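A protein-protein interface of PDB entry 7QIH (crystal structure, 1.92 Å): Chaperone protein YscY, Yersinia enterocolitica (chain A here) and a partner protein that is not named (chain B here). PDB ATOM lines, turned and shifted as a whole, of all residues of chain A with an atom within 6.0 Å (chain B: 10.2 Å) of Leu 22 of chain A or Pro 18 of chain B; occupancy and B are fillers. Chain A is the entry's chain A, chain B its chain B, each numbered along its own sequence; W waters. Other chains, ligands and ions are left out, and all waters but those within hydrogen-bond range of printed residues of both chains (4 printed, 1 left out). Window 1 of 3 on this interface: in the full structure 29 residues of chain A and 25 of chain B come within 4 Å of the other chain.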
ATOM      1  N   GLN A  17     -16.118   1.157  -2.926  1.00  0.00           N
ATOM      2  CA  GLN A  17     -16.929   0.945  -4.121  1.00  0.00           C
ATOM      3  C   GLN A  17     -16.632   1.996  -5.183  1.00  0.00           C
ATOM      4  O   GLN A  17     -16.584   1.681  -6.378  1.00  0.00           O
ATOM      5  CB  GLN A  17     -18.412   0.941  -3.753  1.00  0.00           C
ATOM      6  CG  GLN A  17     -18.834  -0.284  -2.954  1.00  0.00           C
ATOM      7  CD  GLN A  17     -20.215  -0.151  -2.342  1.00  0.00           C
ATOM      8  OE1 GLN A  17     -20.703   0.955  -2.114  1.00  0.00           O
ATOM      9  NE2 GLN A  17     -20.852  -1.284  -2.072  1.00  0.00           N
ATOM     10  N   GLN A  18     -16.433   3.252  -4.773  1.00  0.00           N
ATOM     11  CA  GLN A  18     -15.986   4.271  -5.718  1.00  0.00           C
ATOM     12  C   GLN A  18     -14.648   3.885  -6.333  1.00  0.00           C
ATOM     13  O   GLN A  18     -14.462   3.966  -7.552  1.00  0.00           O
ATOM     14  CB  GLN A  18     -15.876   5.630  -5.019  1.00  0.00           C
ATOM     15  CG  GLN A  18     -17.170   6.131  -4.400  1.00  0.00           C
ATOM     16  CD  GLN A  18     -16.963   7.357  -3.529  1.00  0.00           C
ATOM     17  OE1 GLN A  18     -16.161   8.236  -3.848  1.00  0.00           O
ATOM     18  NE2 GLN A  18     -17.685   7.418  -2.415  1.00  0.00           N
ATOM     19  N   GLU A  19     -13.700   3.464  -5.493  1.00  0.00           N
ATOM     20  CA  GLU A  19     -12.398   3.032  -5.989  1.00  0.00           C
ATOM     21  C   GLU A  19     -12.532   1.855  -6.948  1.00  0.00           C
ATOM     22  O   GLU A  19     -11.860   1.811  -7.987  1.00  0.00           O
ATOM     23  CB  GLU A  19     -11.500   2.660  -4.811  1.00  0.00           C
ATOM     24  CG  GLU A  19     -10.117   2.198  -5.196  1.00  0.00           C
ATOM     25  CD  GLU A  19      -9.324   1.725  -3.998  1.00  0.00           C
ATOM     26  OE1 GLU A  19      -9.575   0.596  -3.525  1.00  0.00           O
ATOM     27  OE2 GLU A  19      -8.466   2.492  -3.516  1.00  0.00           O
ATOM     28  N   PHE A  20     -13.392   0.892  -6.612  1.00  0.00           N
ATOM     29  CA  PHE A  20     -13.585  -0.276  -7.466  1.00  0.00           C
ATOM     30  C   PHE A  20     -13.982   0.136  -8.878  1.00  0.00           C
ATOM     31  O   PHE A  20     -13.416  -0.352  -9.863  1.00  0.00           O
ATOM     32  CB  PHE A  20     -14.643  -1.198  -6.853  1.00  0.00           C
ATOM     33  CG  PHE A  20     -14.858  -2.474  -7.622  1.00  0.00           C
ATOM     34  CD1 PHE A  20     -15.768  -2.530  -8.666  1.00  0.00           C
ATOM     35  CD2 PHE A  20     -14.155  -3.618  -7.292  1.00  0.00           C
ATOM     36  CE1 PHE A  20     -15.964  -3.700  -9.372  1.00  0.00           C
ATOM     37  CE2 PHE A  20     -14.350  -4.791  -7.991  1.00  0.00           C
ATOM     38  CZ  PHE A  20     -15.254  -4.831  -9.033  1.00  0.00           C
ATOM     39  N   LEU A  21     -14.952   1.047  -8.996  1.00  0.00           N
ATOM     40  CA  LEU A  21     -15.393   1.486 -10.316  1.00  0.00           C
ATOM     41  C   LEU A  21     -14.307   2.281 -11.029  1.00  0.00           C
ATOM     42  O   LEU A  21     -14.091   2.100 -12.234  1.00  0.00           O
ATOM     43  CB  LEU A  21     -16.674   2.314 -10.194  1.00  0.00           C
ATOM     44  CG  LEU A  21     -17.926   1.539  -9.773  1.00  0.00           C
ATOM     45  CD1 LEU A  21     -19.095   2.490  -9.549  1.00  0.00           C
ATOM     46  CD2 LEU A  21     -18.279   0.481 -10.813  1.00  0.00           C
ATOM     47  N   LEU A  22     -13.620   3.169 -10.306  1.00  0.00           N
ATOM     48  CA  LEU A  22     -12.569   3.980 -10.914  1.00  0.00           C
ATOM     49  C   LEU A  22     -11.454   3.110 -11.481  1.00  0.00           C
ATOM     50  O   LEU A  22     -11.062   3.262 -12.645  1.00  0.00           O
ATOM     51  CB  LEU A  22     -12.003   4.962  -9.885  1.00  0.00           C
ATOM     52  CG  LEU A  22     -10.722   5.691 -10.301  1.00  0.00           C
ATOM     53  CD1 LEU A  22     -11.028   6.784 -11.319  1.00  0.00           C
ATOM     54  CD2 LEU A  22      -9.983   6.260  -9.087  1.00  0.00           C
ATOM     55  N   LEU A  23     -10.928   2.190 -10.669  1.00  0.00           N
ATOM     56  CA  LEU A  23      -9.762   1.418 -11.087  1.00  0.00           C
ATOM     57  C   LEU A  23     -10.127   0.374 -12.136  1.00  0.00           C
ATOM     58  O   LEU A  23      -9.347   0.121 -13.061  1.00  0.00           O
ATOM     59  CB  LEU A  23      -9.106   0.765  -9.871  1.00  0.00           C
ATOM     60  CG  LEU A  23      -8.497   1.740  -8.859  1.00  0.00           C
ATOM     61  CD1 LEU A  23      -7.838   0.986  -7.716  1.00  0.00           C
ATOM     62  CD2 LEU A  23      -7.495   2.665  -9.537  1.00  0.00           C
ATOM     63  N   ASN A  24     -11.299  -0.250 -12.014  1.00  0.00           N
ATOM     64  CA  ASN A  24     -11.740  -1.161 -13.066  1.00  0.00           C
ATOM     65  C   ASN A  24     -11.958  -0.417 -14.376  1.00  0.00           C
ATOM     66  O   ASN A  24     -11.624  -0.928 -15.452  1.00  0.00           O
ATOM     67  CB  ASN A  24     -13.014  -1.890 -12.641  1.00  0.00           C
ATOM     68  CG  ASN A  24     -12.729  -3.096 -11.778  1.00  0.00           C
ATOM     69  OD1 ASN A  24     -12.383  -4.164 -12.282  1.00  0.00           O
ATOM     70  ND2 ASN A  24     -12.873  -2.938 -10.468  1.00  0.00           N
ATOM     71  N   GLY A  25     -12.507   0.797 -14.309  1.00  0.00           N
ATOM     72  CA  GLY A  25     -12.667   1.586 -15.521  1.00  0.00           C
ATOM     73  C   GLY A  25     -11.336   1.968 -16.141  1.00  0.00           C
ATOM     74  O   GLY A  25     -11.150   1.876 -17.356  1.00  0.00           O
ATOM     75  N   TRP A  26     -10.387   2.400 -15.307  1.00  0.00           N
ATOM     76  CA  TRP A  26      -9.071   2.783 -15.812  1.00  0.00           C
ATOM     77  C   TRP A  26      -8.335   1.589 -16.407  1.00  0.00           C
ATOM     78  O   TRP A  26      -7.719   1.699 -17.473  1.00  0.00           O
ATOM     79  CB  TRP A  26      -8.253   3.425 -14.687  1.00  0.00           C
ATOM     80  CG  TRP A  26      -6.783   3.560 -14.974  1.00  0.00           C
ATOM     81  CD1 TRP A  26      -5.760   2.966 -14.293  1.00  0.00           C
ATOM     82  CD2 TRP A  26      -6.174   4.340 -16.011  1.00  0.00           C
ATOM     83  NE1 TRP A  26      -4.552   3.327 -14.841  1.00  0.00           N
ATOM     84  CE2 TRP A  26      -4.779   4.170 -15.897  1.00  0.00           C
ATOM     85  CE3 TRP A  26      -6.671   5.164 -17.025  1.00  0.00           C
ATOM     86  CZ2 TRP A  26      -3.878   4.792 -16.758  1.00  0.00           C
ATOM     87  CZ3 TRP A  26      -5.775   5.782 -17.877  1.00  0.00           C
ATOM     88  CH2 TRP A  26      -4.394   5.592 -17.738  1.00  0.00           C
ATOM     89  N   LEU A  27      -8.395   0.436 -15.740  1.00  0.00           N
ATOM     90  CA  LEU A  27      -7.701  -0.743 -16.253  1.00  0.00           C
ATOM     91  C   LEU A  27      -8.359  -1.262 -17.526  1.00  0.00           C
ATOM     92  O   LEU A  27      -7.663  -1.663 -18.468  1.00  0.00           O
ATOM     93  CB  LEU A  27      -7.648  -1.830 -15.179  1.00  0.00           C
ATOM     94  CG  LEU A  27      -6.746  -1.494 -13.987  1.00  0.00           C
ATOM     95  CD1 LEU A  27      -6.781  -2.595 -12.940  1.00  0.00           C
ATOM     96  CD2 LEU A  27      -5.320  -1.235 -14.448  1.00  0.00           C
ATOM     97  N   LEU A  41     -17.441   4.025 -15.547  1.00  0.00           N
ATOM     98  CA  LEU A  41     -17.184   5.387 -15.084  1.00  0.00           C
ATOM     99  C   LEU A  41     -18.443   6.245 -15.121  1.00  0.00           C
ATOM    100  O   LEU A  41     -18.595   7.147 -14.289  1.00  0.00           O
ATOM    101  CB  LEU A  41     -16.071   6.025 -15.915  1.00  0.00           C
ATOM    102  CG  LEU A  41     -14.710   5.331 -15.800  1.00  0.00           C
ATOM    103  CD1 LEU A  41     -13.722   5.875 -16.819  1.00  0.00           C
ATOM    104  CD2 LEU A  41     -14.150   5.451 -14.388  1.00  0.00           C
ATOM    105  N   LEU A  44     -20.145   5.407 -11.820  1.00  0.00           N
ATOM    106  CA  LEU A  44     -19.474   6.112 -10.734  1.00  0.00           C
ATOM    107  C   LEU A  44     -19.877   7.579 -10.697  1.00  0.00           C
ATOM    108  O   LEU A  44     -20.238   8.112  -9.642  1.00  0.00           O
ATOM    109  CB  LEU A  44     -17.959   5.976 -10.890  1.00  0.00           C
ATOM    110  CG  LEU A  44     -17.094   6.894 -10.027  1.00  0.00           C
ATOM    111  CD1 LEU A  44     -17.335   6.624  -8.551  1.00  0.00           C
ATOM    112  CD2 LEU A  44     -15.625   6.708 -10.377  1.00  0.00           C
ATOM    113  N   HIS A  51     -16.454  13.214  -8.241  1.00  0.00           N
ATOM    114  CA  HIS A  51     -15.273  12.350  -8.234  1.00  0.00           C
ATOM    115  C   HIS A  51     -14.341  12.800  -9.351  1.00  0.00           C
ATOM    116  O   HIS A  51     -14.514  12.420 -10.512  1.00  0.00           O
ATOM    117  CB  HIS A  51     -15.685  10.893  -8.401  1.00  0.00           C
ATOM    118  CG  HIS A  51     -14.621   9.913  -8.013  1.00  0.00           C
ATOM    119  ND1 HIS A  51     -13.431   9.796  -8.698  1.00  0.00           N
ATOM    120  CD2 HIS A  51     -14.575   8.997  -7.019  1.00  0.00           C
ATOM    121  CE1 HIS A  51     -12.696   8.850  -8.140  1.00  0.00           C
ATOM    122  NE2 HIS A  51     -13.369   8.346  -7.121  1.00  0.00           N
ATOM    123  N   ALA A  53     -11.044  12.340 -10.158  1.00  0.00           N
ATOM    124  CA  ALA A  53     -10.229  11.367 -10.880  1.00  0.00           C
ATOM    125  C   ALA A  53     -11.071  10.569 -11.868  1.00  0.00           C
ATOM    126  O   ALA A  53     -10.628  10.288 -12.988  1.00  0.00           O
ATOM    127  CB  ALA A  53      -9.521  10.434  -9.898  1.00  0.00           C
ATOM    128  N   GLY A  54     -12.295  10.206 -11.477  1.00  0.00           N
ATOM    129  CA  GLY A  54     -13.177   9.515 -12.404  1.00  0.00           C
ATOM    130  C   GLY A  54     -13.544  10.367 -13.604  1.00  0.00           C
ATOM    131  O   GLY A  54     -13.613   9.870 -14.731  1.00  0.00           O
ATOM    132  N   ARG A  55     -13.782  11.661 -13.377  1.00  0.00           N
ATOM    133  CA  ARG A  55     -14.080  12.570 -14.480  1.00  0.00           C
ATOM    134  C   ARG A  55     -12.930  12.629 -15.476  1.00  0.00           C
ATOM    135  O   ARG A  55     -13.152  12.591 -16.692  1.00  0.00           O
ATOM    136  CB  ARG A  55     -14.375  13.968 -13.940  1.00  0.00           C
ATOM    137  CG  ARG A  55     -15.670  14.089 -13.170  1.00  0.00           C
ATOM    138  CD  ARG A  55     -16.790  14.584 -14.067  1.00  0.00           C
ATOM    139  NE  ARG A  55     -18.005  14.855 -13.311  1.00  0.00           N
ATOM    140  CZ  ARG A  55     -19.129  15.319 -13.840  1.00  0.00           C
ATOM    141  NH1 ARG A  55     -19.224  15.590 -15.131  1.00  0.00           N
ATOM    142  NH2 ARG A  55     -20.183  15.512 -13.053  1.00  0.00           N
ATOM    143  N   CYS A  57     -10.580  10.325 -15.990  1.00  0.00           N
ATOM    144  CA  CYS A  57     -10.484   9.054 -16.696  1.00  0.00           C
ATOM    145  C   CYS A  57     -11.538   8.954 -17.794  1.00  0.00           C
ATOM    146  O   CYS A  57     -11.232   8.540 -18.918  1.00  0.00           O
ATOM    147  CB  CYS A  57     -10.615   7.898 -15.705  1.00  0.00           C
ATOM    148  SG  CYS A  57      -9.963   6.333 -16.307  1.00  0.00           S
ATOM    149  N   LEU B  12      -1.778  13.168 -21.878  1.00  0.00           N
ATOM    150  CA  LEU B  12      -3.191  12.886 -21.631  1.00  0.00           C
ATOM    151  C   LEU B  12      -3.361  11.609 -20.817  1.00  0.00           C
ATOM    152  O   LEU B  12      -4.117  11.579 -19.837  1.00  0.00           O
ATOM    153  CB  LEU B  12      -3.946  12.778 -22.957  1.00  0.00           C
ATOM    154  CG  LEU B  12      -4.322  14.085 -23.656  1.00  0.00           C
ATOM    155  CD1 LEU B  12      -4.991  13.802 -24.993  1.00  0.00           C
ATOM    156  CD2 LEU B  12      -5.232  14.911 -22.765  1.00  0.00           C
ATOM    157  N   TRP B  13      -2.672  10.536 -21.214  1.00  0.00           N
ATOM    158  CA  TRP B  13      -2.763   9.282 -20.469  1.00  0.00           C
ATOM    159  C   TRP B  13      -2.257   9.448 -19.041  1.00  0.00           C
ATOM    160  O   TRP B  13      -2.825   8.875 -18.104  1.00  0.00           O
ATOM    161  CB  TRP B  13      -1.988   8.180 -21.191  1.00  0.00           C
ATOM    162  CG  TRP B  13      -2.743   7.571 -22.335  1.00  0.00           C
ATOM    163  CD1 TRP B  13      -2.549   7.805 -23.666  1.00  0.00           C
ATOM    164  CD2 TRP B  13      -3.822   6.631 -22.246  1.00  0.00           C
ATOM    165  NE1 TRP B  13      -3.437   7.065 -24.410  1.00  0.00           N
ATOM    166  CE2 TRP B  13      -4.229   6.336 -23.563  1.00  0.00           C
ATOM    167  CE3 TRP B  13      -4.481   6.009 -21.181  1.00  0.00           C
ATOM    168  CZ2 TRP B  13      -5.266   5.446 -23.843  1.00  0.00           C
ATOM    169  CZ3 TRP B  13      -5.511   5.125 -21.461  1.00  0.00           C
ATOM    170  CH2 TRP B  13      -5.892   4.853 -22.780  1.00  0.00           C
ATOM    171  N   ASP B  14      -1.190  10.230 -18.855  1.00  0.00           N
ATOM    172  CA  ASP B  14      -0.711  10.509 -17.505  1.00  0.00           C
ATOM    173  C   ASP B  14      -1.745  11.295 -16.713  1.00  0.00           C
ATOM    174  O   ASP B  14      -1.891  11.102 -15.499  1.00  0.00           O
ATOM    175  CB  ASP B  14       0.616  11.269 -17.556  1.00  0.00           C
ATOM    176  CG  ASP B  14       1.739  10.445 -18.154  1.00  0.00           C
ATOM    177  OD1 ASP B  14       1.652   9.198 -18.126  1.00  0.00           O
ATOM    178  OD2 ASP B  14       2.715  11.047 -18.651  1.00  0.00           O
ATOM    179  N   PHE B  15      -2.478  12.185 -17.386  1.00  0.00           N
ATOM    180  CA  PHE B  15      -3.528  12.949 -16.720  1.00  0.00           C
ATOM    181  C   PHE B  15      -4.710  12.059 -16.354  1.00  0.00           C
ATOM    182  O   PHE B  15      -5.325  12.236 -15.296  1.00  0.00           O
ATOM    183  CB  PHE B  15      -3.977  14.097 -17.625  1.00  0.00           C
ATOM    184  CG  PHE B  15      -4.856  15.106 -16.949  1.00  0.00           C
ATOM    185  CD1 PHE B  15      -4.390  15.836 -15.869  1.00  0.00           C
ATOM    186  CD2 PHE B  15      -6.136  15.349 -17.415  1.00  0.00           C
ATOM    187  CE1 PHE B  15      -5.195  16.776 -15.252  1.00  0.00           C
ATOM    188  CE2 PHE B  15      -6.942  16.288 -16.805  1.00  0.00           C
ATOM    189  CZ  PHE B  15      -6.470  17.004 -15.725  1.00  0.00           C
ATOM    190  N   ALA B  16      -5.043  11.097 -17.215  1.00  0.00           N
ATOM    191  CA  ALA B  16      -6.160  10.204 -16.924  1.00  0.00           C
ATOM    192  C   ALA B  16      -5.821   9.212 -15.821  1.00  0.00           C
ATOM    193  O   ALA B  16      -6.722   8.739 -15.121  1.00  0.00           O
ATOM    194  CB  ALA B  16      -6.578   9.453 -18.187  1.00  0.00           C
ATOM    195  N   SER B  17      -4.547   8.884 -15.655  1.00  0.00           N
ATOM    196  CA  SER B  17      -4.160   7.852 -14.706  1.00  0.00           C
ATOM    197  C   SER B  17      -4.510   8.283 -13.285  1.00  0.00           C
ATOM    198  O   SER B  17      -4.156   9.397 -12.874  1.00  0.00           O
ATOM    199  CB  SER B  17      -2.664   7.564 -14.813  1.00  0.00           C
ATOM    200  OG  SER B  17      -2.281   6.557 -13.893  1.00  0.00           O
ATOM    201  N   PRO B  18      -5.206   7.447 -12.508  1.00  0.00           N
ATOM    202  CA  PRO B  18      -5.452   7.788 -11.099  1.00  0.00           C
ATOM    203  C   PRO B  18      -4.198   7.767 -10.240  1.00  0.00           C
ATOM    204  O   PRO B  18      -4.230   8.293  -9.119  1.00  0.00           O
ATOM    205  CB  PRO B  18      -6.461   6.721 -10.649  1.00  0.00           C
ATOM    206  CG  PRO B  18      -6.265   5.589 -11.591  1.00  0.00           C
ATOM    207  CD  PRO B  18      -5.883   6.202 -12.905  1.00  0.00           C
ATOM    208  N   GLY B  19      -3.100   7.185 -10.721  1.00  0.00           N
ATOM    209  CA  GLY B  19      -1.842   7.221 -10.002  1.00  0.00           C
ATOM    210  C   GLY B  19      -1.671   6.165  -8.936  1.00  0.00           C
ATOM    211  O   GLY B  19      -0.668   6.196  -8.215  1.00  0.00           O
ATOM    212  N   TYR B  20      -2.615   5.240  -8.807  1.00  0.00           N
ATOM    213  CA  TYR B  20      -2.512   4.142  -7.857  1.00  0.00           C
ATOM    214  C   TYR B  20      -3.352   2.989  -8.388  1.00  0.00           C
ATOM    215  O   TYR B  20      -4.025   3.109  -9.415  1.00  0.00           O
ATOM    216  CB  TYR B  20      -2.957   4.575  -6.454  1.00  0.00           C
ATOM    217  CG  TYR B  20      -4.428   4.921  -6.335  1.00  0.00           C
ATOM    218  CD1 TYR B  20      -4.926   6.112  -6.845  1.00  0.00           C
ATOM    219  CD2 TYR B  20      -5.314   4.063  -5.695  1.00  0.00           C
ATOM    220  CE1 TYR B  20      -6.266   6.434  -6.733  1.00  0.00           C
ATOM    221  CE2 TYR B  20      -6.656   4.377  -5.577  1.00  0.00           C
ATOM    222  CZ  TYR B  20      -7.126   5.565  -6.097  1.00  0.00           C
ATOM    223  OH  TYR B  20      -8.461   5.881  -5.980  1.00  0.00           O
ATOM    224  N   THR B  21      -3.309   1.861  -7.687  1.00  0.00           N
ATOM    225  CA  THR B  21      -4.097   0.700  -8.077  1.00  0.00           C
ATOM    226  C   THR B  21      -4.582   0.002  -6.810  1.00  0.00           C
ATOM    227  O   THR B  21      -4.448   0.528  -5.700  1.00  0.00           O
ATOM    228  CB  THR B  21      -3.288  -0.228  -8.992  1.00  0.00           C
ATOM    229  OG1 THR B  21      -4.156  -1.233  -9.533  1.00  0.00           O
ATOM    230  CG2 THR B  21      -2.152  -0.895  -8.222  1.00  0.00           C
ATOM    231  N   PHE B  22      -5.164  -1.185  -6.981  1.00  0.00           N
ATOM    232  CA  PHE B  22      -5.717  -1.920  -5.852  1.00  0.00           C
ATOM    233  C   PHE B  22      -4.636  -2.213  -4.820  1.00  0.00           C
ATOM    234  O   PHE B  22      -3.506  -2.570  -5.161  1.00  0.00           O
ATOM    235  CB  PHE B  22      -6.367  -3.218  -6.331  1.00  0.00           C
ATOM    236  CG  PHE B  22      -7.562  -3.001  -7.214  1.00  0.00           C
ATOM    237  CD1 PHE B  22      -8.784  -2.642  -6.669  1.00  0.00           C
ATOM    238  CD2 PHE B  22      -7.463  -3.155  -8.587  1.00  0.00           C
ATOM    239  CE1 PHE B  22      -9.888  -2.437  -7.478  1.00  0.00           C
ATOM    240  CE2 PHE B  22      -8.562  -2.952  -9.403  1.00  0.00           C
ATOM    241  CZ  PHE B  22      -9.777  -2.593  -8.847  1.00  0.00           C
ATOM    242  N   HIS B  23      -4.993  -2.052  -3.547  1.00  0.00           N
ATOM    243  CA  HIS B  23      -4.040  -2.123  -2.449  1.00  0.00           C
ATOM    244  C   HIS B  23      -4.674  -2.886  -1.294  1.00  0.00           C
ATOM    245  O   HIS B  23      -5.843  -3.279  -1.347  1.00  0.00           O
ATOM    246  CB  HIS B  23      -3.605  -0.718  -2.015  1.00  0.00           C
ATOM    247  CG  HIS B  23      -4.749   0.214  -1.767  1.00  0.00           C
ATOM    248  ND1 HIS B  23      -5.316   0.383  -0.521  1.00  0.00           N
ATOM    249  CD2 HIS B  23      -5.446   1.016  -2.607  1.00  0.00           C
ATOM    250  CE1 HIS B  23      -6.306   1.253  -0.605  1.00  0.00           C
ATOM    251  NE2 HIS B  23      -6.406   1.653  -1.860  1.00  0.00           N
ATOM    252  N   TYR B  31     -11.457  -7.813  -3.789  1.00  0.00           N
ATOM    253  CA  TYR B  31     -12.011  -7.536  -5.111  1.00  0.00           C
ATOM    254  C   TYR B  31     -13.304  -8.310  -5.337  1.00  0.00           C
ATOM    255  O   TYR B  31     -14.326  -7.730  -5.717  1.00  0.00           O
ATOM    256  CB  TYR B  31     -10.991  -7.867  -6.202  1.00  0.00           C
ATOM    257  CG  TYR B  31     -11.447  -7.484  -7.596  1.00  0.00           C
ATOM    258  CD1 TYR B  31     -12.263  -8.330  -8.342  1.00  0.00           C
ATOM    259  CD2 TYR B  31     -11.064  -6.277  -8.169  1.00  0.00           C
ATOM    260  CE1 TYR B  31     -12.687  -7.983  -9.611  1.00  0.00           C
ATOM    261  CE2 TYR B  31     -11.480  -5.923  -9.443  1.00  0.00           C
ATOM    262  CZ  TYR B  31     -12.292  -6.780 -10.158  1.00  0.00           C
ATOM    263  OH  TYR B  31     -12.712  -6.440 -11.423  1.00  0.00           O
ATOM    264  N   LEU B  38     -21.249  -4.839  -5.063  1.00  0.00           N
ATOM    265  CA  LEU B  38     -21.625  -3.722  -5.923  1.00  0.00           C
ATOM    266  C   LEU B  38     -22.641  -4.142  -6.979  1.00  0.00           C
ATOM    267  O   LEU B  38     -23.541  -3.365  -7.320  1.00  0.00           O
ATOM    268  CB  LEU B  38     -20.378  -3.129  -6.576  1.00  0.00           C
ATOM    269  CG  LEU B  38     -20.511  -1.772  -7.269  1.00  0.00           C
ATOM    270  CD1 LEU B  38     -21.137  -0.745  -6.339  1.00  0.00           C
ATOM    271  CD2 LEU B  38     -19.147  -1.303  -7.737  1.00  0.00           C
ATOM    272  N   LEU B  42     -26.137  -2.153  -7.299  1.00  0.00           N
ATOM    273  CA  LEU B  42     -26.553  -1.419  -8.489  1.00  0.00           C
ATOM    274  C   LEU B  42     -27.749  -2.060  -9.187  1.00  0.00           C
ATOM    275  O   LEU B  42     -28.425  -1.384  -9.972  1.00  0.00           O
ATOM    276  CB  LEU B  42     -25.383  -1.299  -9.470  1.00  0.00           C
ATOM    277  CG  LEU B  42     -24.108  -0.594  -8.996  1.00  0.00           C
ATOM    278  CD1 LEU B  42     -23.104  -0.484 -10.135  1.00  0.00           C
ATOM    279  CD2 LEU B  42     -24.411   0.779  -8.415  1.00  0.00           C
ATOM    280  N   LEU B  57     -20.979  -6.255 -14.569  1.00  0.00           N
ATOM    281  CA  LEU B  57     -20.267  -6.915 -13.480  1.00  0.00           C
ATOM    282  C   LEU B  57     -20.734  -8.357 -13.304  1.00  0.00           C
ATOM    283  O   LEU B  57     -19.919  -9.255 -13.065  1.00  0.00           O
ATOM    284  CB  LEU B  57     -20.453  -6.125 -12.185  1.00  0.00           C
ATOM    285  CG  LEU B  57     -19.905  -4.694 -12.205  1.00  0.00           C
ATOM    286  CD1 LEU B  57     -20.277  -3.956 -10.926  1.00  0.00           C
ATOM    287  CD2 LEU B  57     -18.396  -4.697 -12.413  1.00  0.00           C
HETATM  288  O   HOH W   1      -7.724  -1.394  -3.153  1.00  0.00           O
HETATM  289  O   HOH W   2     -11.719   6.350  -5.795  1.00  0.00           O
HETATM  290  O   HOH W   3      -7.988   9.722 -12.925  1.00  0.00           O
HETATM  291  O   HOH W   4      -2.164   4.441 -12.677  1.00  0.00           O
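Water W4 lies within hydrogen-bond range of OG of Ser 17 of chain B (2.4 Å), NE1 of Trp 26 of chain A (3.4 Å) and N of Gly 19 of chain B (3.5 Å).
Water W3 bridges O of Ala 53 of chain A (2.7 Å) and O of Ala 16 of chain B (2.7 Å).
Water W1 bridges OE1 of Glu 19 of chain A and N of His 23 of chain B.
Water W2 lies within hydrogen-bond range of a ring nitrogen (NE2) of His 51 of chain A (2.9 Å) and the side-chain hydroxyl of Tyr 20 of chain B (3.3 Å).
OG of Ser 17 of chain B lies close to N of Gly 19 of chain B (3.3 Å).
O of Phe 20 of chain A lies within hydrogen-bond range of ND2 of Asn 24 of chain A (2.7 Å).
Hydrophobic or aromatic side chains of chain B within 4 Å of the printed part of chain A: Trp 13, Ala 16, Pro 18, Tyr 20, Phe 22, His 23, Tyr 31 and Leu 38.
Among the printed residues, no Asp or Glu carboxylate lies within 4 Å of a Lys or Arg side-chain nitrogen of the other chain.
The side-chain amide oxygen (OD1) of Asn 24 of chain A lies within hydrogen-bond range of the side-chain hydroxyl (OH) of Tyr 31 of chain B, 2.5 Å away.
NE2 of His 23 of chain B is in hydrogen-bond range of OE2 of Glu 19 of chain A, 2.8 Å away.
Among the printed residues, merely in contact across the chains: Glu 19 of chain A with Tyr 20 of chain B (3.3 Å), Phe 20 of chain A with Tyr 31 of chain B (3.4 Å), Trp 26 of chain A with Trp 13 of chain B (3.5 Å), Trp 26 of chain A with Pro 18 of chain B (3.5 Å), Leu 22 of chain A with Tyr 20 of chain B (3.5 Å), Leu 23 of chain A with Tyr 20 of chain B (3.5 Å), Asn 24 of chain A with Phe 22 of chain B (3.5 Å), Leu 23 of chain A with Thr 21 of chain B (3.5 Å), Leu 23 of chain A with Phe 22 of chain B (3.5 Å), Trp 26 of chain A with Ser 17 of chain B (3.6 Å), Leu 21 of chain A with Leu 38 of chain B (3.7 Å), Phe 20 of chain A with Leu 38 of chain B (3.7 Å), Trp 26 of chain A with Ala 16 of chain B (3.8 Å), Leu 23 of chain A with Pro 18 of chain B (3.8 Å), Leu 22 of chain A with Pro 18 of chain B (3.9 Å) and Leu 27 of chain A with Phe 22 of chain B (3.98 Å).
Printed residues of chain B within 4 Å of Phe 20 of chain A: Tyr 31 and Leu 38.
Leu 21 of chain A touches just one residue of chain B: Leu 38.
Leu 23 of chain A touches four residues of chain B.
Of the printed residues of chain B, Asn 24 of chain A touches Phe 22 and Tyr 31.
Gly 25 of chain A touches none of the printed residues of chain B.
Of chain B, only Trp 13, Ala 16, Ser 17 and Pro 18 come within 4 Å of Trp 26 of chain A.
No residue of chain B comes within 4 Å of Gly 54 of chain A.
Of the printed residues of chain A, Trp 13 of chain B touches Trp 26 (3.5 Å).
Printed residues of chain A within 4 Å of Ser 17 of chain B: Trp 26.
Pro 18 of chain B touches just these residues of chain A: Leu 22, Leu 23 and Trp 26.
Of the printed residues of chain A, Thr 21 of chain B touches Leu 23 (3.5 Å).
The nearest printed residue of chain A that does not touch Ala 16 of chain B is Cys 57 of chain A (4.03 Å).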
